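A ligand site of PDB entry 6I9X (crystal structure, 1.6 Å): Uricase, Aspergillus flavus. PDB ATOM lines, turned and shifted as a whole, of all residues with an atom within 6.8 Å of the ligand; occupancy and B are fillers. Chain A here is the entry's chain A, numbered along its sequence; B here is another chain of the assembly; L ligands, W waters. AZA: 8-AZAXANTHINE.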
ATOM      1  N   SER A 158      27.667 -35.875 -27.975  1.00  0.00           N
ATOM      2  CA  SER A 158      26.900 -34.614 -27.969  1.00  0.00           C
ATOM      3  C   SER A 158      25.445 -34.971 -28.270  1.00  0.00           C
ATOM      4  O   SER A 158      25.186 -35.729 -29.219  1.00  0.00           O
ATOM      5  CB  SER A 158      27.444 -33.582 -28.951  1.00  0.00           C
ATOM      6  OG  SER A 158      26.603 -32.445 -29.018  1.00  0.00           O
ATOM      7  N   GLN A 159      24.544 -34.424 -27.495  1.00  0.00           N
ATOM      8  CA  GLN A 159      23.101 -34.638 -27.608  1.00  0.00           C
ATOM      9  C   GLN A 159      22.417 -33.281 -27.645  1.00  0.00           C
ATOM     10  O   GLN A 159      22.964 -32.267 -27.117  1.00  0.00           O
ATOM     11  CB  GLN A 159      22.559 -35.438 -26.410  1.00  0.00           C
ATOM     12  CG  GLN A 159      23.384 -36.678 -26.147  1.00  0.00           C
ATOM     13  CD  GLN A 159      22.826 -37.602 -25.091  1.00  0.00           C
ATOM     14  OE1 GLN A 159      21.784 -37.361 -24.488  1.00  0.00           O
ATOM     15  NE2 GLN A 159      23.542 -38.680 -24.858  1.00  0.00           N
ATOM     16  N   PHE A 160      21.211 -33.277 -28.147  1.00  0.00           N
ATOM     17  CA  PHE A 160      20.324 -32.119 -28.040  1.00  0.00           C
ATOM     18  C   PHE A 160      18.884 -32.543 -28.218  1.00  0.00           C
ATOM     19  O   PHE A 160      18.381 -32.735 -29.321  1.00  0.00           O
ATOM     20  CB  PHE A 160      20.746 -30.997 -29.002  1.00  0.00           C
ATOM     21  CG  PHE A 160      20.064 -29.690 -28.666  1.00  0.00           C
ATOM     22  CD1 PHE A 160      20.283 -29.063 -27.446  1.00  0.00           C
ATOM     23  CD2 PHE A 160      19.166 -29.068 -29.534  1.00  0.00           C
ATOM     24  CE1 PHE A 160      19.638 -27.904 -27.108  1.00  0.00           C
ATOM     25  CE2 PHE A 160      18.533 -27.893 -29.186  1.00  0.00           C
ATOM     26  CZ  PHE A 160      18.731 -27.321 -27.962  1.00  0.00           C
ATOM     27  N   PHE A 163      14.126 -29.718 -26.090  1.00  0.00           N
ATOM     28  CA  PHE A 163      13.904 -28.284 -26.286  1.00  0.00           C
ATOM     29  C   PHE A 163      12.445 -27.986 -26.636  1.00  0.00           C
ATOM     30  O   PHE A 163      11.640 -28.911 -26.918  1.00  0.00           O
ATOM     31  CB  PHE A 163      14.845 -27.738 -27.381  1.00  0.00           C
ATOM     32  CG  PHE A 163      14.827 -28.557 -28.633  1.00  0.00           C
ATOM     33  CD1 PHE A 163      15.720 -29.600 -28.803  1.00  0.00           C
ATOM     34  CD2 PHE A 163      13.954 -28.243 -29.655  1.00  0.00           C
ATOM     35  CE1 PHE A 163      15.729 -30.368 -29.959  1.00  0.00           C
ATOM     36  CE2 PHE A 163      13.946 -29.009 -30.795  1.00  0.00           C
ATOM     37  CZ  PHE A 163      14.797 -30.065 -30.943  1.00  0.00           C
ATOM     38  N   LEU A 171      13.363 -28.767 -36.102  1.00  0.00           N
ATOM     39  CA  LEU A 171      14.559 -29.523 -35.680  1.00  0.00           C
ATOM     40  C   LEU A 171      14.175 -30.828 -34.962  1.00  0.00           C
ATOM     41  O   LEU A 171      13.312 -30.793 -34.059  1.00  0.00           O
ATOM     42  CB  LEU A 171      15.361 -28.632 -34.724  1.00  0.00           C
ATOM     43  CG  LEU A 171      16.670 -29.252 -34.194  1.00  0.00           C
ATOM     44  CD1 LEU A 171      17.683 -29.441 -35.291  1.00  0.00           C
ATOM     45  CD2 LEU A 171      17.247 -28.384 -33.090  1.00  0.00           C
ATOM     46  N   ARG A 177      25.232 -36.395 -32.050  1.00  0.00           N
ATOM     47  CA  ARG A 177      25.533 -35.430 -33.125  1.00  0.00           C
ATOM     48  C   ARG A 177      27.009 -35.059 -33.025  1.00  0.00           C
ATOM     49  O   ARG A 177      27.679 -35.287 -32.029  1.00  0.00           O
ATOM     50  CB  ARG A 177      24.622 -34.222 -33.042  1.00  0.00           C
ATOM     51  CG  ARG A 177      24.921 -33.333 -31.836  1.00  0.00           C
ATOM     52  CD  ARG A 177      23.984 -32.162 -31.723  1.00  0.00           C
ATOM     53  NE  ARG A 177      24.372 -31.366 -30.565  1.00  0.00           N
ATOM     54  CZ  ARG A 177      23.965 -30.110 -30.330  1.00  0.00           C
ATOM     55  NH1 ARG A 177      23.055 -29.533 -31.098  1.00  0.00           N
ATOM     56  NH2 ARG A 177      24.413 -29.463 -29.265  1.00  0.00           N
ATOM     57  N   LEU A 179      29.610 -32.000 -32.563  1.00  0.00           N
ATOM     58  CA  LEU A 179      29.690 -30.670 -31.946  1.00  0.00           C
ATOM     59  C   LEU A 179      31.044 -30.081 -32.306  1.00  0.00           C
ATOM     60  O   LEU A 179      32.115 -30.652 -32.054  1.00  0.00           O
ATOM     61  CB  LEU A 179      29.508 -30.809 -30.428  1.00  0.00           C
ATOM     62  CG  LEU A 179      29.535 -29.492 -29.672  1.00  0.00           C
ATOM     63  CD1 LEU A 179      28.415 -28.600 -30.135  1.00  0.00           C
ATOM     64  CD2 LEU A 179      29.415 -29.744 -28.168  1.00  0.00           C
ATOM     65  N   SER A 225      27.710 -34.114 -23.678  1.00  0.00           N
ATOM     66  CA  SER A 225      27.130 -32.765 -23.687  1.00  0.00           C
ATOM     67  C   SER A 225      25.624 -32.836 -23.896  1.00  0.00           C
ATOM     68  O   SER A 225      25.168 -33.347 -24.909  1.00  0.00           O
ATOM     69  CB  SER A 225      27.827 -31.951 -24.783  1.00  0.00           C
ATOM     70  OG  SER A 225      27.203 -30.712 -24.893  1.00  0.00           O
ATOM     71  N   ALA A 226      24.870 -32.143 -23.063  1.00  0.00           N
ATOM     72  CA  ALA A 226      23.422 -32.038 -23.172  1.00  0.00           C
ATOM     73  C   ALA A 226      23.042 -30.867 -24.073  1.00  0.00           C
ATOM     74  O   ALA A 226      21.892 -30.764 -24.499  1.00  0.00           O
ATOM     75  CB  ALA A 226      22.842 -31.841 -21.782  1.00  0.00           C
ATOM     76  N   SER A 227      24.006 -29.956 -24.274  1.00  0.00           N
ATOM     77  CA  SER A 227      23.797 -28.711 -25.047  1.00  0.00           C
ATOM     78  C   SER A 227      25.120 -27.971 -24.989  1.00  0.00           C
ATOM     79  O   SER A 227      25.909 -28.194 -24.073  1.00  0.00           O
ATOM     80  CB  SER A 227      22.688 -27.826 -24.541  1.00  0.00           C
ATOM     81  OG  SER A 227      22.989 -27.332 -23.232  1.00  0.00           O
ATOM     82  N   VAL A 228      25.308 -26.983 -25.863  1.00  0.00           N
ATOM     83  CA  VAL A 228      26.476 -26.100 -25.729  1.00  0.00           C
ATOM     84  C   VAL A 228      26.376 -25.352 -24.390  1.00  0.00           C
ATOM     85  O   VAL A 228      27.395 -25.218 -23.717  1.00  0.00           O
ATOM     86  CB  VAL A 228      26.514 -25.155 -26.928  1.00  0.00           C
ATOM     87  CG1 VAL A 228      27.608 -24.134 -26.738  1.00  0.00           C
ATOM     88  CG2 VAL A 228      26.722 -25.951 -28.218  1.00  0.00           C
ATOM     89  N   GLN A 229      25.188 -24.868 -24.066  1.00  0.00           N
ATOM     90  CA  GLN A 229      24.895 -24.121 -22.817  1.00  0.00           C
ATOM     91  C   GLN A 229      25.450 -24.914 -21.630  1.00  0.00           C
ATOM     92  O   GLN A 229      26.175 -24.357 -20.754  1.00  0.00           O
ATOM     93  CB  GLN A 229      23.389 -23.936 -22.703  1.00  0.00           C
ATOM     94  CG  GLN A 229      22.773 -22.898 -23.638  1.00  0.00           C
ATOM     95  CD  GLN A 229      22.311 -23.407 -24.991  1.00  0.00           C
ATOM     96  OE1 GLN A 229      22.827 -24.391 -25.509  1.00  0.00           O
ATOM     97  NE2 GLN A 229      21.395 -22.616 -25.576  1.00  0.00           N
ATOM     98  N   ASN A 255      28.027 -22.556 -32.731  1.00  0.00           N
ATOM     99  CA  ASN A 255      27.658 -23.961 -32.919  1.00  0.00           C
ATOM    100  C   ASN A 255      27.805 -24.171 -34.443  1.00  0.00           C
ATOM    101  O   ASN A 255      26.962 -23.642 -35.146  1.00  0.00           O
ATOM    102  CB  ASN A 255      26.284 -24.242 -32.318  1.00  0.00           C
ATOM    103  CG  ASN A 255      25.968 -25.723 -32.337  1.00  0.00           C
ATOM    104  OD1 ASN A 255      26.801 -26.542 -32.738  1.00  0.00           O
ATOM    105  ND2 ASN A 255      24.746 -26.075 -31.957  1.00  0.00           N
ATOM    106  N   HIS A 257      27.498 -26.103 -37.557  1.00  0.00           N
ATOM    107  CA  HIS A 257      26.631 -27.257 -37.855  1.00  0.00           C
ATOM    108  C   HIS A 257      27.242 -28.129 -38.934  1.00  0.00           C
ATOM    109  O   HIS A 257      27.748 -27.634 -39.955  1.00  0.00           O
ATOM    110  CB  HIS A 257      25.242 -26.782 -38.245  1.00  0.00           C
ATOM    111  CG  HIS A 257      24.597 -25.891 -37.239  1.00  0.00           C
ATOM    112  ND1 HIS A 257      24.273 -26.311 -35.953  1.00  0.00           N
ATOM    113  CD2 HIS A 257      24.266 -24.580 -37.295  1.00  0.00           C
ATOM    114  CE1 HIS A 257      23.735 -25.299 -35.291  1.00  0.00           C
ATOM    115  NE2 HIS A 257      23.725 -24.212 -36.088  1.00  0.00           N
ATOM    116  N   GLY A 287      24.691 -21.283 -34.847  1.00  0.00           N
ATOM    117  CA  GLY A 287      24.278 -20.936 -33.487  1.00  0.00           C
ATOM    118  C   GLY A 287      25.332 -20.089 -32.824  1.00  0.00           C
ATOM    119  O   GLY A 287      26.518 -20.172 -33.171  1.00  0.00           O
ATOM    120  N   ILE A 289      26.148 -18.939 -28.779  1.00  0.00           N
ATOM    121  CA  ILE A 289      25.743 -19.185 -27.386  1.00  0.00           C
ATOM    122  C   ILE A 289      26.741 -18.442 -26.495  1.00  0.00           C
ATOM    123  O   ILE A 289      27.949 -18.660 -26.648  1.00  0.00           O
ATOM    124  CB  ILE A 289      25.749 -20.683 -27.067  1.00  0.00           C
ATOM    125  CG1 ILE A 289      25.153 -21.577 -28.167  1.00  0.00           C
ATOM    126  CG2 ILE A 289      25.045 -20.879 -25.716  1.00  0.00           C
ATOM    127  CD1 ILE A 289      23.830 -21.237 -28.546  1.00  0.00           C
ATOM    128  N   TYR B   9      21.641 -16.120 -26.327  1.00  0.00           N
ATOM    129  CA  TYR B   9      21.935 -17.166 -27.314  1.00  0.00           C
ATOM    130  C   TYR B   9      20.996 -16.944 -28.503  1.00  0.00           C
ATOM    131  O   TYR B   9      19.940 -16.305 -28.409  1.00  0.00           O
ATOM    132  CB  TYR B   9      21.840 -18.553 -26.712  1.00  0.00           C
ATOM    133  CG  TYR B   9      20.430 -19.042 -26.689  1.00  0.00           C
ATOM    134  CD1 TYR B   9      19.483 -18.493 -25.853  1.00  0.00           C
ATOM    135  CD2 TYR B   9      19.962 -19.905 -27.661  1.00  0.00           C
ATOM    136  CE1 TYR B   9      18.124 -18.784 -25.973  1.00  0.00           C
ATOM    137  CE2 TYR B   9      18.641 -20.265 -27.754  1.00  0.00           C
ATOM    138  CZ  TYR B   9      17.711 -19.707 -26.902  1.00  0.00           C
ATOM    139  OH  TYR B   9      16.386 -20.021 -27.044  1.00  0.00           O
ATOM    140  N   GLY B  10      21.413 -17.454 -29.652  1.00  0.00           N
ATOM    141  CA  GLY B  10      20.555 -17.404 -30.818  1.00  0.00           C
ATOM    142  C   GLY B  10      21.268 -17.825 -32.076  1.00  0.00           C
ATOM    143  O   GLY B  10      22.078 -18.703 -32.039  1.00  0.00           O
ATOM    144  N   LYS B  11      20.902 -17.205 -33.188  1.00  0.00           N
ATOM    145  CA  LYS B  11      21.415 -17.619 -34.519  1.00  0.00           C
ATOM    146  C   LYS B  11      22.053 -16.406 -35.171  1.00  0.00           C
ATOM    147  O   LYS B  11      21.493 -15.332 -35.161  1.00  0.00           O
ATOM    148  CB  LYS B  11      20.285 -18.123 -35.415  1.00  0.00           C
ATOM    149  CG  LYS B  11      20.736 -19.010 -36.538  1.00  0.00           C
ATOM    150  CD  LYS B  11      21.305 -20.308 -36.053  1.00  0.00           C
ATOM    151  CE  LYS B  11      20.728 -21.537 -36.661  1.00  0.00           C
ATOM    152  NZ  LYS B  11      21.171 -22.766 -35.944  1.00  0.00           N
ATOM    153  N   ASN B  52      16.680 -28.250 -21.125  1.00  0.00           N
ATOM    154  CA  ASN B  52      16.471 -27.671 -22.481  1.00  0.00           C
ATOM    155  C   ASN B  52      15.030 -27.169 -22.680  1.00  0.00           C
ATOM    156  O   ASN B  52      14.740 -26.592 -23.713  1.00  0.00           O
ATOM    157  CB  ASN B  52      16.942 -28.655 -23.560  1.00  0.00           C
ATOM    158  CG  ASN B  52      18.439 -28.861 -23.548  1.00  0.00           C
ATOM    159  OD1 ASN B  52      19.179 -27.992 -23.077  1.00  0.00           O
ATOM    160  ND2 ASN B  52      18.915 -29.992 -24.050  1.00  0.00           N
ATOM    161  N   ILE B  55      14.646 -23.651 -23.857  1.00  0.00           N
ATOM    162  CA  ILE B  55      15.365 -23.242 -25.098  1.00  0.00           C
ATOM    163  C   ILE B  55      14.438 -23.259 -26.325  1.00  0.00           C
ATOM    164  O   ILE B  55      13.942 -24.327 -26.708  1.00  0.00           O
ATOM    165  CB  ILE B  55      16.621 -24.087 -25.351  1.00  0.00           C
ATOM    166  CG1 ILE B  55      17.644 -23.950 -24.221  1.00  0.00           C
ATOM    167  CG2 ILE B  55      17.256 -23.654 -26.690  1.00  0.00           C
ATOM    168  CD1 ILE B  55      18.827 -24.893 -24.389  1.00  0.00           C
ATOM    169  N   VAL B  56      14.240 -22.088 -26.889  1.00  0.00           N
ATOM    170  CA  VAL B  56      13.732 -21.925 -28.270  1.00  0.00           C
ATOM    171  C   VAL B  56      14.929 -22.282 -29.154  1.00  0.00           C
ATOM    172  O   VAL B  56      15.935 -21.547 -29.048  1.00  0.00           O
ATOM    173  CB  VAL B  56      13.212 -20.497 -28.470  1.00  0.00           C
ATOM    174  CG1 VAL B  56      12.789 -20.272 -29.901  1.00  0.00           C
ATOM    175  CG2 VAL B  56      12.062 -20.228 -27.499  1.00  0.00           C
ATOM    176  N   ALA B  57      14.901 -23.389 -29.866  1.00  0.00           N
ATOM    177  CA  ALA B  57      16.107 -23.862 -30.594  1.00  0.00           C
ATOM    178  C   ALA B  57      16.588 -22.767 -31.551  1.00  0.00           C
ATOM    179  O   ALA B  57      15.788 -22.076 -32.142  1.00  0.00           O
ATOM    180  CB  ALA B  57      15.832 -25.134 -31.353  1.00  0.00           C
ATOM    181  N   THR B  58      17.909 -22.670 -31.716  1.00  0.00           N
ATOM    182  CA  THR B  58      18.466 -21.661 -32.646  1.00  0.00           C
ATOM    183  C   THR B  58      17.942 -21.983 -34.057  1.00  0.00           C
ATOM    184  O   THR B  58      17.673 -21.043 -34.796  1.00  0.00           O
ATOM    185  CB  THR B  58      19.992 -21.566 -32.571  1.00  0.00           C
ATOM    186  OG1 THR B  58      20.540 -22.774 -33.087  1.00  0.00           O
ATOM    187  CG2 THR B  58      20.462 -21.307 -31.156  1.00  0.00           C
ATOM    188  N   ASP B  59      17.774 -23.253 -34.395  1.00  0.00           N
ATOM    189  CA  ASP B  59      17.170 -23.650 -35.687  1.00  0.00           C
ATOM    190  C   ASP B  59      15.786 -23.013 -35.840  1.00  0.00           C
ATOM    191  O   ASP B  59      15.438 -22.568 -36.932  1.00  0.00           O
ATOM    192  CB  ASP B  59      17.098 -25.157 -35.785  1.00  0.00           C
ATOM    193  CG  ASP B  59      16.755 -25.581 -37.207  1.00  0.00           C
ATOM    194  OD1 ASP B  59      17.696 -25.561 -38.053  1.00  0.00           O
ATOM    195  OD2 ASP B  59      15.571 -25.887 -37.443  1.00  0.00           O
ATOM    196  N   SER B  60      14.977 -23.003 -34.779  1.00  0.00           N
ATOM    197  CA  SER B  60      13.631 -22.365 -34.818  1.00  0.00           C
ATOM    198  C   SER B  60      13.727 -20.870 -34.992  1.00  0.00           C
ATOM    199  O   SER B  60      12.834 -20.253 -35.615  1.00  0.00           O
ATOM    200  CB  SER B  60      12.846 -22.741 -33.551  1.00  0.00           C
ATOM    201  OG  SER B  60      12.858 -24.126 -33.404  1.00  0.00           O
HETATM  202  N1  AZA L   1      22.005 -25.348 -28.172  1.00  0.00           N
HETATM  203  C2  AZA L   1      22.607 -26.441 -28.718  1.00  0.00           C
HETATM  204  O2  AZA L   1      23.525 -26.999 -28.171  1.00  0.00           O
HETATM  205  N3  AZA L   1      22.179 -26.861 -29.953  1.00  0.00           N
HETATM  206  C4  AZA L   1      21.138 -26.254 -30.533  1.00  0.00           C
HETATM  207  C5  AZA L   1      20.510 -25.181 -29.953  1.00  0.00           C
HETATM  208  C6  AZA L   1      20.926 -24.668 -28.683  1.00  0.00           C
HETATM  209  O6  AZA L   1      20.495 -23.672 -28.096  1.00  0.00           O
HETATM  210  N7  AZA L   1      19.511 -24.777 -30.789  1.00  0.00           N
HETATM  211  N8  AZA L   1      19.506 -25.560 -31.824  1.00  0.00           N
HETATM  212  N9  AZA L   1      20.489 -26.459 -31.708  1.00  0.00           N
HETATM  213  O   HOH W   1      21.271 -28.171 -33.737  1.00  0.00           O
HETATM  214  O   HOH W   2      22.940 -23.730 -32.024  1.00  0.00           O
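N of Thr 58 of chain B is in hydrogen-bond range of N7 of the ligand.
A nitrogen (N7) of the ligand is in hydrogen-bond range of the side-chain hydroxyl of Thr 58 of chain B (3.2 Å).
An oxygen (O2) of the ligand lies within hydrogen-bond range of the guanidinium group of Arg 177, at 2.8 Å.
An oxygen (O6) of the ligand lies within hydrogen-bond range of the side-chain amide nitrogen (NE2) of Gln 229, 2.9 Å away.
The backbone NH (N) of Val 228 is in hydrogen-bond range of an oxygen (O2) of the ligand (2.9 Å).
A nitrogen (N3) of the ligand lies close to the side-chain amide nitrogen of Asn 255.
OG1 of Thr 58 of chain B is in hydrogen-bond range of NZ of Lys 11 of chain B, 2.9 Å away.
O of Ser 158 sits at hydrogen-bond distance from N of Arg 177.
The side-chain hydroxyl of Ser 227 sits close to the backbone NH of Gln 229, at 3.4 Å.
The backbone carbonyl oxygen (O) of Asn 255 is in hydrogen-bond range of a ring nitrogen (NE2) of His 257, 3.4 Å away.
N of Asn 255 is in hydrogen-bond range of O of Gly 287.
The backbone carbonyl oxygen (O) of Ser 227 sits at hydrogen-bond distance from the side-chain hydroxyl (OG) of Ser 225, 2.9 Å away.
The backbone carbonyl oxygen (O) of Val 56 of chain B is in hydrogen-bond range of the side-chain hydroxyl (OH) of Tyr 9 of chain B (2.6 Å).
Phe 160 touches the ligand (CE2 to C4, 3.4 Å).
CD2 of Leu 171 touches N8 of the ligand, at 3.8 Å.
CA of Ser 227 touches O2 of the ligand (3.6 Å).
CD2 of Tyr 9 of chain B touches O6 of the ligand, 3.8 Å away.
CG2 of Ile 55 of chain B touches O6 of the ligand, at 3.5 Å.
Ala 57 of chain B touches the ligand.
N of Asp 59 of chain B touches N8 of the ligand, 3.9 Å away.
Hydrophobic or aromatic side chains that line the ligand: Phe 160, Leu 171, Val 228, Tyr 9 of chain B, Ile 55 of chain B and Ala 57 of chain B.
Of the 26 residues printed, 12 come within 4 Å of the ligand.
The nearest printed residue that does not touch the ligand is Ile 289 (4.2 Å).
Water W1 lies within hydrogen-bond range of N9 of the ligand and NH1 of Arg 177.
Water W2 bridges the side-chain hydroxyl of Thr 58 of chain B (2.8 Å) and the side-chain amide nitrogen of Asn 255 (3.0 Å).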
